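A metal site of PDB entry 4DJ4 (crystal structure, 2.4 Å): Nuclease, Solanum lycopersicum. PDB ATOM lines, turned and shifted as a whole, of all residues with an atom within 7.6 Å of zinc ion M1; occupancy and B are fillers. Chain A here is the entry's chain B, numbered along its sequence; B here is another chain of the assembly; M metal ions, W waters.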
ATOM      1  N   TRP A   1      16.273 -14.002 -18.612  1.00  0.00           N
ATOM      2  CA  TRP A   1      15.273 -15.035 -18.224  1.00  0.00           C
ATOM      3  C   TRP A   1      13.849 -14.573 -18.484  1.00  0.00           C
ATOM      4  O   TRP A   1      13.563 -13.389 -18.539  1.00  0.00           O
ATOM      5  CB  TRP A   1      15.415 -15.396 -16.741  1.00  0.00           C
ATOM      6  CG  TRP A   1      16.761 -15.951 -16.334  1.00  0.00           C
ATOM      7  CD1 TRP A   1      17.693 -15.368 -15.458  1.00  0.00           C
ATOM      8  CD2 TRP A   1      17.372 -17.218 -16.744  1.00  0.00           C
ATOM      9  NE1 TRP A   1      18.801 -16.178 -15.309  1.00  0.00           N
ATOM     10  CE2 TRP A   1      18.689 -17.283 -16.050  1.00  0.00           C
ATOM     11  CE3 TRP A   1      16.996 -18.266 -17.585  1.00  0.00           C
ATOM     12  CZ2 TRP A   1      19.525 -18.358 -16.200  1.00  0.00           C
ATOM     13  CZ3 TRP A   1      17.877 -19.343 -17.731  1.00  0.00           C
ATOM     14  CH2 TRP A   1      19.113 -19.377 -17.069  1.00  0.00           C
ATOM     15  N   SER A   2      12.927 -15.507 -18.624  1.00  0.00           N
ATOM     16  CA  SER A   2      11.487 -15.186 -18.518  1.00  0.00           C
ATOM     17  C   SER A   2      11.156 -15.172 -17.038  1.00  0.00           C
ATOM     18  O   SER A   2      12.059 -15.280 -16.175  1.00  0.00           O
ATOM     19  CB  SER A   2      10.651 -16.206 -19.289  1.00  0.00           C
ATOM     20  OG  SER A   2      10.960 -16.192 -20.685  1.00  0.00           O
ATOM     21  N   HIS A   6      13.759 -15.335 -13.242  1.00  0.00           N
ATOM     22  CA  HIS A   6      13.914 -14.175 -12.376  1.00  0.00           C
ATOM     23  C   HIS A   6      13.408 -14.439 -10.992  1.00  0.00           C
ATOM     24  O   HIS A   6      14.125 -14.124 -10.023  1.00  0.00           O
ATOM     25  CB  HIS A   6      13.329 -12.875 -13.004  1.00  0.00           C
ATOM     26  CG  HIS A   6      14.069 -12.420 -14.240  1.00  0.00           C
ATOM     27  ND1 HIS A   6      15.292 -11.819 -14.178  1.00  0.00           N
ATOM     28  CD2 HIS A   6      13.736 -12.549 -15.613  1.00  0.00           C
ATOM     29  CE1 HIS A   6      15.743 -11.599 -15.454  1.00  0.00           C
ATOM     30  NE2 HIS A   6      14.780 -12.034 -16.332  1.00  0.00           N
ATOM     31  N   ASP A  45      10.908  -6.148 -17.171  1.00  0.00           N
ATOM     32  CA  ASP A  45      10.531  -6.745 -18.472  1.00  0.00           C
ATOM     33  C   ASP A  45       9.195  -6.146 -18.929  1.00  0.00           C
ATOM     34  O   ASP A  45       8.956  -6.054 -20.127  1.00  0.00           O
ATOM     35  CB  ASP A  45      10.526  -8.288 -18.443  1.00  0.00           C
ATOM     36  CG  ASP A  45      11.909  -8.912 -18.868  1.00  0.00           C
ATOM     37  OD1 ASP A  45      12.682  -8.259 -19.590  1.00  0.00           O
ATOM     38  OD2 ASP A  45      12.222 -10.067 -18.480  1.00  0.00           O
ATOM     39  N   ARG A  48      10.232  -1.979 -19.772  1.00  0.00           N
ATOM     40  CA  ARG A  48      11.073  -1.740 -20.957  1.00  0.00           C
ATOM     41  C   ARG A  48      10.270  -1.370 -22.215  1.00  0.00           C
ATOM     42  O   ARG A  48      10.836  -0.872 -23.183  1.00  0.00           O
ATOM     43  CB  ARG A  48      11.953  -2.975 -21.276  1.00  0.00           C
ATOM     44  CG  ARG A  48      11.170  -4.176 -21.813  1.00  0.00           C
ATOM     45  CD  ARG A  48      12.022  -5.417 -22.122  1.00  0.00           C
ATOM     46  NE  ARG A  48      12.989  -5.185 -23.186  1.00  0.00           N
ATOM     47  CZ  ARG A  48      13.982  -6.021 -23.529  1.00  0.00           C
ATOM     48  NH1 ARG A  48      14.152  -7.190 -22.892  1.00  0.00           N
ATOM     49  NH2 ARG A  48      14.810  -5.681 -24.511  1.00  0.00           N
ATOM     50  N   HIS A  60      19.079  -5.059 -20.860  1.00  0.00           N
ATOM     51  CA  HIS A  60      18.742  -6.461 -20.603  1.00  0.00           C
ATOM     52  C   HIS A  60      19.803  -7.415 -21.123  1.00  0.00           C
ATOM     53  O   HIS A  60      19.860  -8.569 -20.658  1.00  0.00           O
ATOM     54  CB  HIS A  60      17.341  -6.770 -21.164  1.00  0.00           C
ATOM     55  CG  HIS A  60      16.254  -6.053 -20.404  1.00  0.00           C
ATOM     56  ND1 HIS A  60      15.547  -6.630 -19.417  1.00  0.00           N
ATOM     57  CD2 HIS A  60      15.857  -4.703 -20.417  1.00  0.00           C
ATOM     58  CE1 HIS A  60      14.718  -5.726 -18.864  1.00  0.00           C
ATOM     59  NE2 HIS A  60      14.910  -4.544 -19.472  1.00  0.00           N
ATOM     60  N   PHE A  61      20.677  -6.944 -22.006  1.00  0.00           N
ATOM     61  CA  PHE A  61      21.602  -7.853 -22.665  1.00  0.00           C
ATOM     62  C   PHE A  61      22.955  -7.209 -23.075  1.00  0.00           C
ATOM     63  O   PHE A  61      23.270  -6.038 -22.755  1.00  0.00           O
ATOM     64  CB  PHE A  61      20.893  -8.465 -23.911  1.00  0.00           C
ATOM     65  CG  PHE A  61      20.476  -7.435 -24.913  1.00  0.00           C
ATOM     66  CD1 PHE A  61      21.385  -6.958 -25.847  1.00  0.00           C
ATOM     67  CD2 PHE A  61      19.215  -6.877 -24.866  1.00  0.00           C
ATOM     68  CE1 PHE A  61      21.031  -5.973 -26.754  1.00  0.00           C
ATOM     69  CE2 PHE A  61      18.842  -5.904 -25.772  1.00  0.00           C
ATOM     70  CZ  PHE A  61      19.755  -5.445 -26.722  1.00  0.00           C
ATOM     71  N   ASP A 126      19.725 -11.571 -15.614  1.00  0.00           N
ATOM     72  CA  ASP A 126      19.856 -11.627 -17.078  1.00  0.00           C
ATOM     73  C   ASP A 126      21.256 -11.822 -17.548  1.00  0.00           C
ATOM     74  O   ASP A 126      21.473 -12.424 -18.609  1.00  0.00           O
ATOM     75  CB  ASP A 126      19.335 -10.323 -17.733  1.00  0.00           C
ATOM     76  CG  ASP A 126      17.829 -10.352 -18.051  1.00  0.00           C
ATOM     77  OD1 ASP A 126      17.228 -11.447 -18.015  1.00  0.00           O
ATOM     78  OD2 ASP A 126      17.273  -9.275 -18.365  1.00  0.00           O
ATOM     79  N   GLN A 129      21.971 -15.433 -17.688  1.00  0.00           N
ATOM     80  CA  GLN A 129      21.336 -16.191 -18.766  1.00  0.00           C
ATOM     81  C   GLN A 129      22.292 -16.133 -19.928  1.00  0.00           C
ATOM     82  O   GLN A 129      22.406 -15.125 -20.588  1.00  0.00           O
ATOM     83  CB  GLN A 129      19.965 -15.597 -19.173  1.00  0.00           C
ATOM     84  CG  GLN A 129      18.908 -16.595 -19.675  1.00  0.00           C
ATOM     85  CD  GLN A 129      19.104 -17.004 -21.123  1.00  0.00           C
ATOM     86  OE1 GLN A 129      20.159 -17.495 -21.503  1.00  0.00           O
ATOM     87  NE2 GLN A 129      18.068 -16.811 -21.950  1.00  0.00           N
ATOM     88  N   MET A 131      22.224 -16.760 -23.035  1.00  0.00           N
ATOM     89  CA  MET A 131      21.871 -16.212 -24.364  1.00  0.00           C
ATOM     90  C   MET A 131      21.587 -14.709 -24.330  1.00  0.00           C
ATOM     91  O   MET A 131      21.397 -14.092 -25.378  1.00  0.00           O
ATOM     92  CB  MET A 131      20.704 -16.957 -25.016  1.00  0.00           C
ATOM     93  CG  MET A 131      20.937 -18.458 -25.217  1.00  0.00           C
ATOM     94  SD  MET A 131      22.340 -18.985 -26.243  1.00  0.00           S
ATOM     95  CE  MET A 131      22.066 -18.097 -27.790  1.00  0.00           C
ATOM     96  N   HIS A 132      21.562 -14.115 -23.134  1.00  0.00           N
ATOM     97  CA  HIS A 132      21.510 -12.660 -22.985  1.00  0.00           C
ATOM     98  C   HIS A 132      22.881 -12.035 -23.227  1.00  0.00           C
ATOM     99  O   HIS A 132      23.047 -10.820 -23.108  1.00  0.00           O
ATOM    100  CB  HIS A 132      21.000 -12.276 -21.611  1.00  0.00           C
ATOM    101  CG  HIS A 132      19.492 -12.141 -21.523  1.00  0.00           C
ATOM    102  ND1 HIS A 132      18.870 -11.023 -21.063  1.00  0.00           N
ATOM    103  CD2 HIS A 132      18.479 -13.031 -21.861  1.00  0.00           C
ATOM    104  CE1 HIS A 132      17.548 -11.197 -21.105  1.00  0.00           C
ATOM    105  NE2 HIS A 132      17.308 -12.430 -21.592  1.00  0.00           N
ATOM    106  N   ALA A 139      20.524 -11.910 -32.552  1.00  0.00           N
ATOM    107  CA  ALA A 139      19.977 -11.307 -31.327  1.00  0.00           C
ATOM    108  C   ALA A 139      19.984 -12.257 -30.110  1.00  0.00           C
ATOM    109  O   ALA A 139      19.002 -12.373 -29.387  1.00  0.00           O
ATOM    110  CB  ALA A 139      18.576 -10.770 -31.612  1.00  0.00           C
ATOM    111  N   GLY A 140      21.112 -12.925 -29.887  1.00  0.00           N
ATOM    112  CA  GLY A 140      21.248 -13.861 -28.767  1.00  0.00           C
ATOM    113  C   GLY A 140      20.340 -15.063 -28.983  1.00  0.00           C
ATOM    114  O   GLY A 140      19.703 -15.546 -28.032  1.00  0.00           O
ATOM    115  N   ASN A 142      17.486 -15.233 -30.486  1.00  0.00           N
ATOM    116  CA  ASN A 142      16.091 -14.856 -30.727  1.00  0.00           C
ATOM    117  C   ASN A 142      15.572 -15.164 -32.147  1.00  0.00           C
ATOM    118  O   ASN A 142      14.427 -15.588 -32.281  1.00  0.00           O
ATOM    119  CB  ASN A 142      15.845 -13.391 -30.367  1.00  0.00           C
ATOM    120  CG  ASN A 142      15.241 -13.234 -28.993  1.00  0.00           C
ATOM    121  OD1 ASN A 142      14.088 -13.605 -28.780  1.00  0.00           O
ATOM    122  ND2 ASN A 142      16.013 -12.684 -28.038  1.00  0.00           N
ATOM    123  N   HIS A 156      16.834 -18.589 -28.161  1.00  0.00           N
ATOM    124  CA  HIS A 156      16.857 -17.678 -27.007  1.00  0.00           C
ATOM    125  C   HIS A 156      15.818 -18.077 -26.005  1.00  0.00           C
ATOM    126  O   HIS A 156      16.110 -18.202 -24.817  1.00  0.00           O
ATOM    127  CB  HIS A 156      16.657 -16.209 -27.432  1.00  0.00           C
ATOM    128  CG  HIS A 156      16.772 -15.259 -26.280  1.00  0.00           C
ATOM    129  ND1 HIS A 156      17.888 -14.563 -26.030  1.00  0.00           N
ATOM    130  CD2 HIS A 156      15.889 -14.981 -25.244  1.00  0.00           C
ATOM    131  CE1 HIS A 156      17.726 -13.862 -24.894  1.00  0.00           C
ATOM    132  NE2 HIS A 156      16.503 -14.114 -24.424  1.00  0.00           N
ATOM    133  N   HIS A 157      14.594 -18.336 -26.484  1.00  0.00           N
ATOM    134  CA  HIS A 157      13.494 -18.728 -25.579  1.00  0.00           C
ATOM    135  C   HIS A 157      13.678 -20.086 -24.901  1.00  0.00           C
ATOM    136  O   HIS A 157      13.248 -20.303 -23.737  1.00  0.00           O
ATOM    137  CB  HIS A 157      12.156 -18.613 -26.325  1.00  0.00           C
ATOM    138  CG  HIS A 157      10.982 -18.533 -25.398  1.00  0.00           C
ATOM    139  ND1 HIS A 157      10.777 -17.474 -24.584  1.00  0.00           N
ATOM    140  CD2 HIS A 157       9.978 -19.465 -25.123  1.00  0.00           C
ATOM    141  CE1 HIS A 157       9.662 -17.697 -23.848  1.00  0.00           C
ATOM    142  NE2 HIS A 157       9.191 -18.916 -24.158  1.00  0.00           N
ATOM    143  N   TRP A 159      16.400 -21.091 -23.646  1.00  0.00           N
ATOM    144  CA  TRP A 159      17.151 -20.745 -22.436  1.00  0.00           C
ATOM    145  C   TRP A 159      16.428 -19.859 -21.484  1.00  0.00           C
ATOM    146  O   TRP A 159      16.545 -20.043 -20.284  1.00  0.00           O
ATOM    147  CB  TRP A 159      18.468 -20.163 -22.845  1.00  0.00           C
ATOM    148  CG  TRP A 159      19.396 -21.217 -23.383  1.00  0.00           C
ATOM    149  CD1 TRP A 159      19.409 -21.793 -24.655  1.00  0.00           C
ATOM    150  CD2 TRP A 159      20.466 -21.893 -22.650  1.00  0.00           C
ATOM    151  NE1 TRP A 159      20.416 -22.716 -24.764  1.00  0.00           N
ATOM    152  CE2 TRP A 159      21.086 -22.832 -23.587  1.00  0.00           C
ATOM    153  CE3 TRP A 159      20.988 -21.787 -21.373  1.00  0.00           C
ATOM    154  CZ2 TRP A 159      22.162 -23.634 -23.227  1.00  0.00           C
ATOM    155  CZ3 TRP A 159      22.063 -22.613 -21.018  1.00  0.00           C
ATOM    156  CH2 TRP A 159      22.621 -23.510 -21.926  1.00  0.00           C
ATOM    157  N   ASP A 160      15.654 -18.872 -21.977  1.00  0.00           N
ATOM    158  CA  ASP A 160      14.865 -18.013 -21.064  1.00  0.00           C
ATOM    159  C   ASP A 160      13.851 -18.833 -20.302  1.00  0.00           C
ATOM    160  O   ASP A 160      13.591 -18.534 -19.110  1.00  0.00           O
ATOM    161  CB  ASP A 160      14.064 -16.918 -21.785  1.00  0.00           C
ATOM    162  CG  ASP A 160      14.791 -15.555 -21.939  1.00  0.00           C
ATOM    163  OD1 ASP A 160      15.693 -15.135 -21.154  1.00  0.00           O
ATOM    164  OD2 ASP A 160      14.361 -14.832 -22.859  1.00  0.00           O
ATOM    165  N   ARG A 161      13.258 -19.838 -20.959  1.00  0.00           N
ATOM    166  CA  ARG A 161      12.059 -20.510 -20.391  1.00  0.00           C
ATOM    167  C   ARG A 161      11.841 -22.021 -20.636  1.00  0.00           C
ATOM    168  O   ARG A 161      11.512 -22.776 -19.724  1.00  0.00           O
ATOM    169  CB  ARG A 161      10.818 -19.774 -20.880  1.00  0.00           C
ATOM    170  CG  ARG A 161       9.706 -19.761 -19.854  1.00  0.00           C
ATOM    171  CD  ARG A 161       8.383 -19.266 -20.391  1.00  0.00           C
ATOM    172  NE  ARG A 161       7.468 -19.201 -19.262  1.00  0.00           N
ATOM    173  CZ  ARG A 161       6.135 -19.277 -19.325  1.00  0.00           C
ATOM    174  NH1 ARG A 161       5.505 -19.393 -20.484  1.00  0.00           N
ATOM    175  NH2 ARG A 161       5.438 -19.236 -18.199  1.00  0.00           N
ATOM    176  N   SER B 107       8.469 -12.444 -22.774  1.00  0.00           N
ATOM    177  CA  SER B 107       8.784 -12.286 -24.199  1.00  0.00           C
ATOM    178  C   SER B 107      10.212 -11.767 -24.313  1.00  0.00           C
ATOM    179  O   SER B 107      10.897 -11.635 -23.288  1.00  0.00           O
ATOM    180  CB  SER B 107       7.797 -11.318 -24.864  1.00  0.00           C
ATOM    181  OG  SER B 107       7.623 -10.130 -24.085  1.00  0.00           O
ATOM    182  N   ASP B 108      10.686 -11.466 -25.523  1.00  0.00           N
ATOM    183  CA  ASP B 108      11.960 -10.752 -25.655  1.00  0.00           C
ATOM    184  C   ASP B 108      12.014  -9.731 -26.791  1.00  0.00           C
ATOM    185  O   ASP B 108      10.978  -9.266 -27.264  1.00  0.00           O
ATOM    186  CB  ASP B 108      13.142 -11.754 -25.687  1.00  0.00           C
ATOM    187  CG  ASP B 108      14.058 -11.613 -24.487  1.00  0.00           C
ATOM    188  OD1 ASP B 108      13.550 -11.291 -23.396  1.00  0.00           O
ATOM    189  OD2 ASP B 108      15.284 -11.789 -24.624  1.00  0.00           O
ATOM    190  N   ARG B 109      13.229  -9.396 -27.208  1.00  0.00           N
ATOM    191  CA  ARG B 109      13.484  -8.279 -28.117  1.00  0.00           C
ATOM    192  C   ARG B 109      12.670  -8.306 -29.396  1.00  0.00           C
ATOM    193  O   ARG B 109      12.418  -7.244 -29.976  1.00  0.00           O
ATOM    194  CB  ARG B 109      14.970  -8.218 -28.512  1.00  0.00           C
ATOM    195  CG  ARG B 109      15.950  -8.808 -27.516  1.00  0.00           C
ATOM    196  CD  ARG B 109      17.094  -7.859 -27.274  1.00  0.00           C
ATOM    197  NE  ARG B 109      17.865  -7.522 -28.474  1.00  0.00           N
ATOM    198  CZ  ARG B 109      19.054  -8.024 -28.792  1.00  0.00           C
ATOM    199  NH1 ARG B 109      19.641  -8.921 -28.001  1.00  0.00           N
ATOM    200  NH2 ARG B 109      19.661  -7.621 -29.902  1.00  0.00           N
HETATM  201 ZN    ZN M   1      15.661 -13.151 -22.810  1.00  0.00          ZN
HETATM  202 ZN    ZN M   2      15.326 -12.053 -18.065  1.00  0.00          ZN
HETATM  203 ZN    ZN M   3      15.182  -8.783 -18.701  1.00  0.00          ZN
HETATM  204  O   HOH W   1      14.542 -12.605 -21.085  1.00  0.00           O
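Zinc ion M1 is bound by NE2 of His 156, 2.1 Å away.
Zinc ion M1 is bound by OD2 of Asp 160.
Water W1 is bound to zinc ion M1.
NE2 of His 132 binds zinc ion M1 (2.2 Å).
Zinc ion M1 is bound by OD2 of Asp 108 of chain B.
Zinc ion M1 is bound by OD1 of Asp 160 (2.6 Å).
Within 4 Å of zinc ion M1: His 132, His 156, Asp 160 and Asp 108 of chain B.
Along chain A the residues within 4 Å of zinc ion M1 span positions 132 to 160.
The nearest printed residue that does not touch zinc ion M1 is Trp 1 (4.3 Å).
ND2 of Asn 142 sits close to ND1 of His 156.
The backbone NH of Asp 160 sits close to the side-chain amide nitrogen of Gln 129 (3.2 Å).
O of Asp 160 is in hydrogen-bond range of N of Ser 2 (3.1 Å).
OD1 of Asp 126 sits close to ND1 of His 132 (3.5 Å).
The backbone carbonyl oxygen (O) of His 60 lies within hydrogen-bond range of a ring nitrogen (ND1) of His 132 (2.7 Å).
O of Gly 140 lies within hydrogen-bond range of ND1 of His 156 (2.9 Å).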
